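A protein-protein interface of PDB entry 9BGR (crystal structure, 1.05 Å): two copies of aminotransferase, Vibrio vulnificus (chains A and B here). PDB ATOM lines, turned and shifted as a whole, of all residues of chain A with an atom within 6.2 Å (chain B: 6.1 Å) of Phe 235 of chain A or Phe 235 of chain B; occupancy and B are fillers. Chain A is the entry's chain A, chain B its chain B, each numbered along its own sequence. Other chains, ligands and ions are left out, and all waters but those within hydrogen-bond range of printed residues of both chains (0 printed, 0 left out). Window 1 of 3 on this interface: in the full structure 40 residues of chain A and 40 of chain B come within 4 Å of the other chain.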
ATOM      1  N   LYS A  16     -13.878   3.308  -8.003  1.00  0.00           N
ATOM      2  CA  LYS A  16     -13.017   2.582  -7.080  1.00  0.00           C
ATOM      3  C   LYS A  16     -12.781   3.389  -5.795  1.00  0.00           C
ATOM      4  O   LYS A  16     -12.834   2.842  -4.697  1.00  0.00           O
ATOM      5  CB  LYS A  16     -11.678   2.246  -7.738  1.00  0.00           C
ATOM      6  CG  LYS A  16     -10.701   1.469  -6.864  1.00  0.00           C
ATOM      7  CD  LYS A  16     -11.214   0.133  -6.370  1.00  0.00           C
ATOM      8  CE  LYS A  16     -11.435  -0.854  -7.497  1.00  0.00           C
ATOM      9  NZ  LYS A  16     -12.132  -2.080  -7.038  1.00  0.00           N
ATOM     10  N   VAL A  17     -12.550   4.699  -5.913  1.00  0.00           N
ATOM     11  CA  VAL A  17     -12.426   5.545  -4.728  1.00  0.00           C
ATOM     12  C   VAL A  17     -13.696   5.429  -3.879  1.00  0.00           C
ATOM     13  O   VAL A  17     -13.632   5.289  -2.658  1.00  0.00           O
ATOM     14  CB  VAL A  17     -12.139   7.011  -5.093  1.00  0.00           C
ATOM     15  CG1 VAL A  17     -12.308   7.926  -3.894  1.00  0.00           C
ATOM     16  CG2 VAL A  17     -10.742   7.194  -5.672  1.00  0.00           C
ATOM     17  N   ILE A  20     -13.774   2.280  -2.028  1.00  0.00           N
ATOM     18  CA  ILE A  20     -12.803   2.254  -0.946  1.00  0.00           C
ATOM     19  C   ILE A  20     -13.365   3.022   0.250  1.00  0.00           C
ATOM     20  O   ILE A  20     -13.310   2.548   1.387  1.00  0.00           O
ATOM     21  CB  ILE A  20     -11.445   2.818  -1.409  1.00  0.00           C
ATOM     22  CG1 ILE A  20     -10.712   1.837  -2.325  1.00  0.00           C
ATOM     23  CG2 ILE A  20     -10.611   3.175  -0.198  1.00  0.00           C
ATOM     24  CD1 ILE A  20      -9.626   2.437  -3.178  1.00  0.00           C
ATOM     25  N   LEU A  21     -13.929   4.206  -0.004  1.00  0.00           N
ATOM     26  CA  LEU A  21     -14.516   5.002   1.060  1.00  0.00           C
ATOM     27  C   LEU A  21     -15.659   4.268   1.759  1.00  0.00           C
ATOM     28  O   LEU A  21     -15.792   4.343   2.981  1.00  0.00           O
ATOM     29  CB  LEU A  21     -14.978   6.357   0.526  1.00  0.00           C
ATOM     30  CG  LEU A  21     -13.890   7.276  -0.028  1.00  0.00           C
ATOM     31  CD1 LEU A  21     -14.483   8.614  -0.406  1.00  0.00           C
ATOM     32  CD2 LEU A  21     -12.742   7.484   0.951  1.00  0.00           C
ATOM     33  N   GLN A  25     -10.227  -0.241   2.635  1.00  0.00           N
ATOM     34  CA  GLN A  25      -9.175   0.230   3.510  1.00  0.00           C
ATOM     35  C   GLN A  25      -8.794   1.639   3.079  1.00  0.00           C
ATOM     36  O   GLN A  25      -8.549   1.887   1.901  1.00  0.00           O
ATOM     37  CB  GLN A  25      -7.975  -0.720   3.437  1.00  0.00           C
ATOM     38  CG  GLN A  25      -6.805  -0.258   4.296  1.00  0.00           C
ATOM     39  CD  GLN A  25      -5.701  -1.269   4.474  1.00  0.00           C
ATOM     40  OE1 GLN A  25      -5.933  -2.439   4.776  1.00  0.00           O
ATOM     41  NE2 GLN A  25      -4.473  -0.822   4.300  1.00  0.00           N
ATOM     42  N   LEU A  26      -8.747   2.561   4.045  1.00  0.00           N
ATOM     43  CA  LEU A  26      -8.429   3.957   3.728  1.00  0.00           C
ATOM     44  C   LEU A  26      -6.929   4.249   3.716  1.00  0.00           C
ATOM     45  O   LEU A  26      -6.471   4.996   2.857  1.00  0.00           O
ATOM     46  CB  LEU A  26      -9.118   4.888   4.729  1.00  0.00           C
ATOM     47  CG  LEU A  26     -10.630   4.736   4.852  1.00  0.00           C
ATOM     48  CD1 LEU A  26     -11.185   5.743   5.847  1.00  0.00           C
ATOM     49  CD2 LEU A  26     -11.342   4.862   3.522  1.00  0.00           C
ATOM     50  N   VAL A  27      -6.172   3.742   4.695  1.00  0.00           N
ATOM     51  CA  VAL A  27      -4.737   3.951   4.697  1.00  0.00           C
ATOM     52  C   VAL A  27      -4.085   3.074   3.636  1.00  0.00           C
ATOM     53  O   VAL A  27      -4.659   2.087   3.172  1.00  0.00           O
ATOM     54  CB  VAL A  27      -4.122   3.670   6.075  1.00  0.00           C
ATOM     55  CG1 VAL A  27      -4.702   4.561   7.145  1.00  0.00           C
ATOM     56  CG2 VAL A  27      -4.227   2.217   6.443  1.00  0.00           C
ATOM     57  N   GLU A  31      -3.993  -0.877  -3.167  1.00  0.00           N
ATOM     58  CA  GLU A  31      -3.868   0.025  -4.298  1.00  0.00           C
ATOM     59  C   GLU A  31      -2.505   0.718  -4.290  1.00  0.00           C
ATOM     60  O   GLU A  31      -1.893   0.881  -5.337  1.00  0.00           O
ATOM     61  CB  GLU A  31      -5.009   1.042  -4.358  1.00  0.00           C
ATOM     62  CG  GLU A  31      -6.353   0.380  -4.562  1.00  0.00           C
ATOM     63  CD  GLU A  31      -6.613  -0.153  -5.959  1.00  0.00           C
ATOM     64  OE1 GLU A  31      -7.381  -1.132  -6.071  1.00  0.00           O
ATOM     65  OE2 GLU A  31      -6.119   0.426  -6.939  1.00  0.00           O
ATOM     66  N   CYS A  32      -2.035   1.168  -3.120  1.00  0.00           N
ATOM     67  CA  CYS A  32      -0.725   1.795  -3.042  1.00  0.00           C
ATOM     68  C   CYS A  32       0.382   0.796  -3.365  1.00  0.00           C
ATOM     69  O   CYS A  32       1.337   1.139  -4.043  1.00  0.00           O
ATOM     70  CB  CYS A  32      -0.468   2.455  -1.700  1.00  0.00           C
ATOM     71  SG  CYS A  32      -1.596   3.860  -1.470  1.00  0.00           S
ATOM     72  N   THR A 189      -2.727  12.734  -8.006  1.00  0.00           N
ATOM     73  CA  THR A 189      -3.506  12.140  -6.936  1.00  0.00           C
ATOM     74  C   THR A 189      -4.056  13.222  -6.010  1.00  0.00           C
ATOM     75  O   THR A 189      -4.404  12.938  -4.866  1.00  0.00           O
ATOM     76  CB  THR A 189      -2.723  11.051  -6.191  1.00  0.00           C
ATOM     77  OG1 THR A 189      -1.612  11.654  -5.511  1.00  0.00           O
ATOM     78  CG2 THR A 189      -2.140   9.984  -7.079  1.00  0.00           C
ATOM     79  N   GLY A 190      -4.148  14.456  -6.517  1.00  0.00           N
ATOM     80  CA  GLY A 190      -4.529  15.619  -5.733  1.00  0.00           C
ATOM     81  C   GLY A 190      -3.316  16.210  -5.025  1.00  0.00           C
ATOM     82  O   GLY A 190      -2.827  17.246  -5.440  1.00  0.00           O
ATOM     83  N   GLU A 191      -2.849  15.508  -4.005  1.00  0.00           N
ATOM     84  CA  GLU A 191      -1.484  15.630  -3.533  1.00  0.00           C
ATOM     85  C   GLU A 191      -0.908  14.226  -3.578  1.00  0.00           C
ATOM     86  O   GLU A 191      -1.603  13.256  -3.272  1.00  0.00           O
ATOM     87  CB  GLU A 191      -1.428  16.148  -2.094  1.00  0.00           C
ATOM     88  CG  GLU A 191      -1.965  17.574  -1.933  1.00  0.00           C
ATOM     89  CD  GLU A 191      -1.001  18.732  -2.150  1.00  0.00           C
ATOM     90  OE1 GLU A 191       0.161  18.517  -2.567  1.00  0.00           O
ATOM     91  OE2 GLU A 191      -1.430  19.878  -1.920  1.00  0.00           O
ATOM     92  N   THR A 233      -2.802   7.923   1.097  1.00  0.00           N
ATOM     93  CA  THR A 233      -3.977   7.082   1.318  1.00  0.00           C
ATOM     94  C   THR A 233      -4.139   6.054   0.197  1.00  0.00           C
ATOM     95  O   THR A 233      -3.676   6.226  -0.918  1.00  0.00           O
ATOM     96  CB  THR A 233      -5.269   7.890   1.446  1.00  0.00           C
ATOM     97  OG1 THR A 233      -5.590   8.494   0.177  1.00  0.00           O
ATOM     98  CG2 THR A 233      -5.215   8.915   2.556  1.00  0.00           C
ATOM     99  N   ASN A 234      -4.877   4.989   0.524  1.00  0.00           N
ATOM    100  CA  ASN A 234      -5.172   3.947  -0.440  1.00  0.00           C
ATOM    101  C   ASN A 234      -6.037   4.471  -1.585  1.00  0.00           C
ATOM    102  O   ASN A 234      -5.872   4.027  -2.711  1.00  0.00           O
ATOM    103  CB  ASN A 234      -5.872   2.788   0.262  1.00  0.00           C
ATOM    104  CG  ASN A 234      -5.845   1.480  -0.495  1.00  0.00           C
ATOM    105  OD1 ASN A 234      -4.825   1.090  -1.046  1.00  0.00           O
ATOM    106  ND2 ASN A 234      -6.972   0.789  -0.500  1.00  0.00           N
ATOM    107  N   PHE A 235      -6.949   5.413  -1.312  1.00  0.00           N
ATOM    108  CA  PHE A 235      -7.789   5.982  -2.360  1.00  0.00           C
ATOM    109  C   PHE A 235      -6.999   6.932  -3.255  1.00  0.00           C
ATOM    110  O   PHE A 235      -7.236   6.977  -4.454  1.00  0.00           O
ATOM    111  CB  PHE A 235      -9.105   6.551  -1.822  1.00  0.00           C
ATOM    112  CG  PHE A 235      -9.012   7.535  -0.693  1.00  0.00           C
ATOM    113  CD1 PHE A 235      -8.985   7.079   0.616  1.00  0.00           C
ATOM    114  CD2 PHE A 235      -8.999   8.900  -0.923  1.00  0.00           C
ATOM    115  CE1 PHE A 235      -8.923   7.962   1.675  1.00  0.00           C
ATOM    116  CE2 PHE A 235      -8.921   9.788   0.141  1.00  0.00           C
ATOM    117  CZ  PHE A 235      -8.905   9.324   1.434  1.00  0.00           C
ATOM    118  N   GLN A 236      -6.032   7.678  -2.711  1.00  0.00           N
ATOM    119  CA  GLN A 236      -5.147   8.446  -3.576  1.00  0.00           C
ATOM    120  C   GLN A 236      -4.344   7.505  -4.470  1.00  0.00           C
ATOM    121  O   GLN A 236      -4.145   7.761  -5.660  1.00  0.00           O
ATOM    122  CB  GLN A 236      -4.242   9.358  -2.750  1.00  0.00           C
ATOM    123  CG  GLN A 236      -4.940  10.598  -2.237  1.00  0.00           C
ATOM    124  CD  GLN A 236      -4.130  11.194  -1.100  1.00  0.00           C
ATOM    125  OE1 GLN A 236      -4.022  10.619  -0.010  1.00  0.00           O
ATOM    126  NE2 GLN A 236      -3.512  12.340  -1.354  1.00  0.00           N
ATOM    127  N   GLY A 237      -3.837   6.414  -3.891  1.00  0.00           N
ATOM    128  CA  GLY A 237      -3.104   5.428  -4.671  1.00  0.00           C
ATOM    129  C   GLY A 237      -3.938   4.856  -5.815  1.00  0.00           C
ATOM    130  O   GLY A 237      -3.429   4.641  -6.919  1.00  0.00           O
ATOM    131  N   ALA A 238      -5.222   4.611  -5.543  1.00  0.00           N
ATOM    132  CA  ALA A 238      -6.130   4.092  -6.560  1.00  0.00           C
ATOM    133  C   ALA A 238      -6.203   5.034  -7.754  1.00  0.00           C
ATOM    134  O   ALA A 238      -6.255   4.605  -8.910  1.00  0.00           O
ATOM    135  CB  ALA A 238      -7.494   3.832  -5.980  1.00  0.00           C
ATOM    136  N   ILE A 239      -6.286   6.339  -7.470  1.00  0.00           N
ATOM    137  CA  ILE A 239      -6.361   7.336  -8.525  1.00  0.00           C
ATOM    138  C   ILE A 239      -5.101   7.234  -9.372  1.00  0.00           C
ATOM    139  O   ILE A 239      -5.136   7.220 -10.608  1.00  0.00           O
ATOM    140  CB  ILE A 239      -6.584   8.744  -7.947  1.00  0.00           C
ATOM    141  CG1 ILE A 239      -7.934   8.868  -7.232  1.00  0.00           C
ATOM    142  CG2 ILE A 239      -6.414   9.796  -9.038  1.00  0.00           C
ATOM    143  CD1 ILE A 239      -8.081  10.132  -6.412  1.00  0.00           C
ATOM    144  N   GLY A 240      -3.937   7.260  -8.705  1.00  0.00           N
ATOM    145  CA  GLY A 240      -2.699   7.349  -9.446  1.00  0.00           C
ATOM    146  C   GLY A 240      -2.492   6.137 -10.341  1.00  0.00           C
ATOM    147  O   GLY A 240      -2.043   6.265 -11.479  1.00  0.00           O
ATOM    148  N   LYS B  16     -19.865  13.864  -2.793  1.00  0.00           N
ATOM    149  CA  LYS B  16     -19.116  15.102  -2.904  1.00  0.00           C
ATOM    150  C   LYS B  16     -17.672  14.843  -3.317  1.00  0.00           C
ATOM    151  O   LYS B  16     -17.118  15.546  -4.159  1.00  0.00           O
ATOM    152  CB  LYS B  16     -19.129  15.813  -1.558  1.00  0.00           C
ATOM    153  CG  LYS B  16     -18.478  17.185  -1.531  1.00  0.00           C
ATOM    154  CD  LYS B  16     -19.010  18.015  -0.375  1.00  0.00           C
ATOM    155  CE  LYS B  16     -20.340  17.516   0.157  1.00  0.00           C
ATOM    156  NZ  LYS B  16     -20.865  18.357   1.261  1.00  0.00           N
ATOM    157  N   VAL B  17     -17.064  13.802  -2.760  1.00  0.00           N
ATOM    158  CA  VAL B  17     -15.728  13.418  -3.196  1.00  0.00           C
ATOM    159  C   VAL B  17     -15.738  13.122  -4.694  1.00  0.00           C
ATOM    160  O   VAL B  17     -14.861  13.592  -5.413  1.00  0.00           O
ATOM    161  CB  VAL B  17     -15.171  12.228  -2.391  1.00  0.00           C
ATOM    162  CG1 VAL B  17     -13.913  11.660  -3.041  1.00  0.00           C
ATOM    163  CG2 VAL B  17     -14.879  12.630  -0.950  1.00  0.00           C
ATOM    164  N   ILE B  20     -15.890  16.262  -6.625  1.00  0.00           N
ATOM    165  CA  ILE B  20     -14.624  16.961  -6.602  1.00  0.00           C
ATOM    166  C   ILE B  20     -13.653  16.304  -7.580  1.00  0.00           C
ATOM    167  O   ILE B  20     -12.969  16.999  -8.336  1.00  0.00           O
ATOM    168  CB  ILE B  20     -14.046  17.028  -5.171  1.00  0.00           C
ATOM    169  CG1 ILE B  20     -14.872  17.969  -4.287  1.00  0.00           C
ATOM    170  CG2 ILE B  20     -12.580  17.425  -5.191  1.00  0.00           C
ATOM    171  CD1 ILE B  20     -14.711  17.742  -2.810  1.00  0.00           C
ATOM    172  N   LEU B  21     -13.558  14.973  -7.556  1.00  0.00           N
ATOM    173  CA  LEU B  21     -12.645  14.310  -8.476  1.00  0.00           C
ATOM    174  C   LEU B  21     -13.003  14.603  -9.927  1.00  0.00           C
ATOM    175  O   LEU B  21     -12.109  14.752 -10.750  1.00  0.00           O
ATOM    176  CB  LEU B  21     -12.599  12.809  -8.210  1.00  0.00           C
ATOM    177  CG  LEU B  21     -12.109  12.419  -6.823  1.00  0.00           C
ATOM    178  CD1 LEU B  21     -12.118  10.929  -6.708  1.00  0.00           C
ATOM    179  CD2 LEU B  21     -10.723  12.972  -6.535  1.00  0.00           C
ATOM    180  N   GLN B  25     -11.868  21.140  -7.524  1.00  0.00           N
ATOM    181  CA  GLN B  25     -10.507  21.439  -7.145  1.00  0.00           C
ATOM    182  C   GLN B  25     -10.005  20.317  -6.246  1.00  0.00           C
ATOM    183  O   GLN B  25     -10.665  19.951  -5.274  1.00  0.00           O
ATOM    184  CB  GLN B  25     -10.461  22.800  -6.448  1.00  0.00           C
ATOM    185  CG  GLN B  25      -9.064  23.158  -5.957  1.00  0.00           C
ATOM    186  CD  GLN B  25      -8.936  24.582  -5.496  1.00  0.00           C
ATOM    187  OE1 GLN B  25      -9.336  25.520  -6.187  1.00  0.00           O
ATOM    188  NE2 GLN B  25      -8.359  24.744  -4.317  1.00  0.00           N
ATOM    189  N   LEU B  26      -8.809  19.802  -6.555  1.00  0.00           N
ATOM    190  CA  LEU B  26      -8.257  18.673  -5.820  1.00  0.00           C
ATOM    191  C   LEU B  26      -7.429  19.126  -4.620  1.00  0.00           C
ATOM    192  O   LEU B  26      -7.518  18.515  -3.558  1.00  0.00           O
ATOM    193  CB  LEU B  26      -7.394  17.816  -6.743  1.00  0.00           C
ATOM    194  CG  LEU B  26      -8.075  17.268  -7.986  1.00  0.00           C
ATOM    195  CD1 LEU B  26      -7.106  16.371  -8.749  1.00  0.00           C
ATOM    196  CD2 LEU B  26      -9.341  16.502  -7.637  1.00  0.00           C
ATOM    197  N   VAL B  27      -6.600  20.172  -4.791  1.00  0.00           N
ATOM    198  CA  VAL B  27      -5.818  20.674  -3.671  1.00  0.00           C
ATOM    199  C   VAL B  27      -6.715  21.463  -2.723  1.00  0.00           C
ATOM    200  O   VAL B  27      -7.802  21.920  -3.082  1.00  0.00           O
ATOM    201  CB  VAL B  27      -4.629  21.529  -4.129  1.00  0.00           C
ATOM    202  CG1 VAL B  27      -3.673  20.761  -5.027  1.00  0.00           C
ATOM    203  CG2 VAL B  27      -5.098  22.821  -4.766  1.00  0.00           C
ATOM    204  N   GLU B  31     -13.617  23.198   0.648  1.00  0.00           N
ATOM    205  CA  GLU B  31     -13.994  22.214   1.650  1.00  0.00           C
ATOM    206  C   GLU B  31     -13.019  22.277   2.833  1.00  0.00           C
ATOM    207  O   GLU B  31     -13.428  22.180   3.981  1.00  0.00           O
ATOM    208  CB  GLU B  31     -14.072  20.805   1.045  1.00  0.00           C
ATOM    209  CG  GLU B  31     -15.170  20.644   0.017  1.00  0.00           C
ATOM    210  CD  GLU B  31     -16.577  20.665   0.568  1.00  0.00           C
ATOM    211  OE1 GLU B  31     -17.466  21.130  -0.169  1.00  0.00           O
ATOM    212  OE2 GLU B  31     -16.806  20.164   1.695  1.00  0.00           O
ATOM    213  N   CYS B  32     -11.721  22.397   2.573  1.00  0.00           N
ATOM    214  CA  CYS B  32     -10.760  22.502   3.648  1.00  0.00           C
ATOM    215  C   CYS B  32     -10.910  23.791   4.431  1.00  0.00           C
ATOM    216  O   CYS B  32     -10.825  23.773   5.648  1.00  0.00           O
ATOM    217  CB  CYS B  32      -9.349  22.401   3.116  1.00  0.00           C
ATOM    218  SG  CYS B  32      -9.011  20.731   2.501  1.00  0.00           S
ATOM    219  N   THR B 189     -10.247  11.085   7.798  1.00  0.00           N
ATOM    220  CA  THR B 189     -10.099  11.492   6.408  1.00  0.00           C
ATOM    221  C   THR B 189      -9.141  10.557   5.687  1.00  0.00           C
ATOM    222  O   THR B 189      -8.583  10.895   4.659  1.00  0.00           O
ATOM    223  CB  THR B 189      -9.683  12.961   6.285  1.00  0.00           C
ATOM    224  OG1 THR B 189      -8.384  13.152   6.852  1.00  0.00           O
ATOM    225  CG2 THR B 189     -10.648  13.914   6.952  1.00  0.00           C
ATOM    226  N   GLY B 190      -9.002   9.343   6.212  1.00  0.00           N
ATOM    227  CA  GLY B 190      -8.055   8.362   5.715  1.00  0.00           C
ATOM    228  C   GLY B 190      -6.678   8.581   6.335  1.00  0.00           C
ATOM    229  O   GLY B 190      -6.254   7.828   7.197  1.00  0.00           O
ATOM    230  N   GLU B 191      -6.022   9.648   5.897  1.00  0.00           N
ATOM    231  CA  GLU B 191      -4.968  10.291   6.672  1.00  0.00           C
ATOM    232  C   GLU B 191      -5.395  11.744   6.790  1.00  0.00           C
ATOM    233  O   GLU B 191      -5.941  12.315   5.846  1.00  0.00           O
ATOM    234  CB  GLU B 191      -3.612  10.249   5.945  1.00  0.00           C
ATOM    235  CG  GLU B 191      -3.047   8.848   5.752  1.00  0.00           C
ATOM    236  CD  GLU B 191      -2.245   8.225   6.895  1.00  0.00           C
ATOM    237  OE1 GLU B 191      -2.086   8.855   7.977  1.00  0.00           O
ATOM    238  OE2 GLU B 191      -1.766   7.077   6.719  1.00  0.00           O
ATOM    239  N   THR B 233      -5.769  17.342   0.972  1.00  0.00           N
ATOM    240  CA  THR B 233      -6.538  17.560  -0.245  1.00  0.00           C
ATOM    241  C   THR B 233      -7.938  18.078   0.080  1.00  0.00           C
ATOM    242  O   THR B 233      -8.473  17.878   1.167  1.00  0.00           O
ATOM    243  CB  THR B 233      -6.666  16.296  -1.101  1.00  0.00           C
ATOM    244  OG1 THR B 233      -7.490  15.347  -0.410  1.00  0.00           O
ATOM    245  CG2 THR B 233      -5.323  15.721  -1.497  1.00  0.00           C
ATOM    246  N   ASN B 234      -8.544  18.719  -0.925  1.00  0.00           N
ATOM    247  CA  ASN B 234      -9.895  19.245  -0.799  1.00  0.00           C
ATOM    248  C   ASN B 234     -10.898  18.103  -0.613  1.00  0.00           C
ATOM    249  O   ASN B 234     -11.867  18.243   0.127  1.00  0.00           O
ATOM    250  CB  ASN B 234     -10.219  20.076  -2.036  1.00  0.00           C
ATOM    251  CG  ASN B 234     -11.384  21.006  -1.853  1.00  0.00           C
ATOM    252  OD1 ASN B 234     -11.513  21.682  -0.836  1.00  0.00           O
ATOM    253  ND2 ASN B 234     -12.230  21.036  -2.864  1.00  0.00           N
ATOM    254  N   PHE B 235     -10.659  16.946  -1.240  1.00  0.00           N
ATOM    255  CA  PHE B 235     -11.593  15.837  -1.087  1.00  0.00           C
ATOM    256  C   PHE B 235     -11.432  15.157   0.276  1.00  0.00           C
ATOM    257  O   PHE B 235     -12.414  14.734   0.874  1.00  0.00           O
ATOM    258  CB  PHE B 235     -11.530  14.854  -2.250  1.00  0.00           C
ATOM    259  CG  PHE B 235     -10.187  14.332  -2.668  1.00  0.00           C
ATOM    260  CD1 PHE B 235      -9.414  15.054  -3.566  1.00  0.00           C
ATOM    261  CD2 PHE B 235      -9.696  13.145  -2.152  1.00  0.00           C
ATOM    262  CE1 PHE B 235      -8.192  14.568  -3.990  1.00  0.00           C
ATOM    263  CE2 PHE B 235      -8.459  12.671  -2.571  1.00  0.00           C
ATOM    264  CZ  PHE B 235      -7.703  13.390  -3.471  1.00  0.00           C
ATOM    265  N   GLN B 236     -10.216  15.087   0.848  1.00  0.00           N
ATOM    266  CA  GLN B 236     -10.119  14.661   2.233  1.00  0.00           C
ATOM    267  C   GLN B 236     -10.850  15.634   3.152  1.00  0.00           C
ATOM    268  O   GLN B 236     -11.485  15.218   4.120  1.00  0.00           O
ATOM    269  CB  GLN B 236      -8.648  14.541   2.636  1.00  0.00           C
ATOM    270  CG  GLN B 236      -7.980  13.291   2.086  1.00  0.00           C
ATOM    271  CD  GLN B 236      -6.480  13.419   2.130  1.00  0.00           C
ATOM    272  OE1 GLN B 236      -5.887  14.187   1.388  1.00  0.00           O
ATOM    273  NE2 GLN B 236      -5.837  12.676   3.018  1.00  0.00           N
ATOM    274  N   GLY B 237     -10.666  16.949   2.931  1.00  0.00           N
ATOM    275  CA  GLY B 237     -11.363  17.938   3.745  1.00  0.00           C
ATOM    276  C   GLY B 237     -12.885  17.749   3.690  1.00  0.00           C
ATOM    277  O   GLY B 237     -13.567  17.866   4.708  1.00  0.00           O
ATOM    278  N   ALA B 238     -13.405  17.413   2.513  1.00  0.00           N
ATOM    279  CA  ALA B 238     -14.835  17.205   2.339  1.00  0.00           C
ATOM    280  C   ALA B 238     -15.310  16.058   3.227  1.00  0.00           C
ATOM    281  O   ALA B 238     -16.390  16.115   3.810  1.00  0.00           O
ATOM    282  CB  ALA B 238     -15.153  16.903   0.905  1.00  0.00           C
ATOM    283  N   ILE B 239     -14.541  14.958   3.289  1.00  0.00           N
ATOM    284  CA  ILE B 239     -14.890  13.812   4.125  1.00  0.00           C
ATOM    285  C   ILE B 239     -14.964  14.260   5.576  1.00  0.00           C
ATOM    286  O   ILE B 239     -15.917  13.979   6.291  1.00  0.00           O
ATOM    287  CB  ILE B 239     -13.891  12.651   3.941  1.00  0.00           C
ATOM    288  CG1 ILE B 239     -13.935  12.103   2.518  1.00  0.00           C
ATOM    289  CG2 ILE B 239     -14.123  11.568   4.997  1.00  0.00           C
ATOM    290  CD1 ILE B 239     -12.787  11.220   2.154  1.00  0.00           C
ATOM    291  N   GLY B 240     -13.914  14.955   6.040  1.00  0.00           N
ATOM    292  CA  GLY B 240     -13.839  15.288   7.448  1.00  0.00           C
ATOM    293  C   GLY B 240     -14.960  16.217   7.893  1.00  0.00           C
ATOM    294  O   GLY B 240     -15.556  16.029   8.957  1.00  0.00           O
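SG of Cys 32 of chain A sits at hydrogen-bond distance from O of Thr 233 of chain A (3.2 Å). The side-chain hydroxyl (OG1) of Thr 189 of chain A is in hydrogen-bond range of the backbone carbonyl oxygen (O) of Glu 191 of chain A (2.8 Å). The side-chain hydroxyl (OG1) of Thr 233 of chain A is in hydrogen-bond range of the side-chain amide oxygen (OE1) of Gln 236 of chain A (2.6 Å). O of Glu 191 of chain B is in hydrogen-bond range of OG1 of Thr 189 of chain B (2.8 Å). The side-chain amide nitrogen (NE2) of Gln 236 of chain B is in hydrogen-bond range of the backbone carbonyl oxygen (O) of Glu 191 of chain B, 2.9 Å away. OG1 of Thr 233 of chain B sits at hydrogen-bond distance from OE1 of Gln 236 of chain B (2.7 Å).
Leu 21 of chain A touches Ile 239 of chain B (CD2 to CD1, 3.9 Å). Gly 190 of chain B touches Leu 26 of chain A (CA to CB, 3.8 Å). Gly 190 of chain A touches Leu 26 of chain B (CA to CB, 3.7 Å). Gly 190 of chain A touches Val 27 of chain B. Glu 191 of chain A touches Val 27 of chain B. CG2 of Thr 233 of chain B touches N of Glu 191 of chain A, at 3.5 Å. N of Glu 191 of chain B touches CG2 of Thr 233 of chain A (3.5 Å). CZ of Phe 235 of chain A touches O of Thr 189 of chain B (3.6 Å). NE2 of Gln 236 of chain A touches CG2 of Thr 233 of chain B, at 3.8 Å. Ile 239 of chain A touches Leu 21 of chain B (CD1 to CD2, 3.9 Å).
Of the printed residues of chain B, Phe 235 of chain A touches Thr 189 (3.6 Å) and Phe 235 (3.98 Å). Of the printed residues of chain A, Phe 235 of chain B touches Thr 189 (3.6 Å) and Phe 235 (3.98 Å). Printed residues of chain B within 4 Å of Leu 21 of chain A: Ile 239 (3.9 Å). Of the printed residues of chain A, Val 27 of chain B touches Gly 190 (3.6 Å) and Glu 191 (3.9 Å). Printed residues of chain A within 4 Å of Leu 26 of chain B: Gly 190. Printed residues of chain A within 4 Å of Thr 189 of chain B: Phe 235. Of the printed residues of chain B, Gln 236 of chain A touches Thr 233 (3.8 Å). Val 17 of chain A touches none of the printed residues of chain B. The nearest printed residue of chain B that does not touch Phe 235 of chain A is Gln 236 of chain B (4.1 Å). The nearest printed residue of chain A that does not touch Phe 235 of chain B is Gln 236 of chain A (4.1 Å).
Printed residues of chain A that touch a printed residue of chain B: Leu 21, Leu 26, Val 27, Thr 189, Gly 190, Glu 191, Thr 233, Phe 235, Gln 236 and Ile 239. Hydrophobic or aromatic side chains of chain A within 4 Å of the printed part of chain B: Leu 21, Leu 26, Val 27, Phe 235 and Ile 239. Of the 20 printed residues of chain B, 10 touch a printed residue of chain A. Hydrophobic or aromatic side chains of chain B within 4 Å of the printed part of chain A: Leu 21, Leu 26, Val 27, Phe 235 and Ile 239. Among the printed residues, 15 pairs touch across the chains. Among the printed residues, no Asp or Glu carboxylate lies within 4 Å of a Lys or Arg side-chain nitrogen of the other chain.
Val 27 of chain A touches Gly 190 of chain B, and with the chains exchanged Gly 190 of chain A touches Val 27 of chain B. Thr 189 of chain A touches Phe 235 of chain B, and with the chains exchanged Phe 235 of chain A touches Thr 189 of chain B. Glu 191 of chain A touches Thr 233 of chain B, and with the chains exchanged Thr 233 of chain A touches Glu 191 of chain B. Thr 233 of chain A touches Gln 236 of chain B, and with the chains exchanged Gln 236 of chain A touches Thr 233 of chain B.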
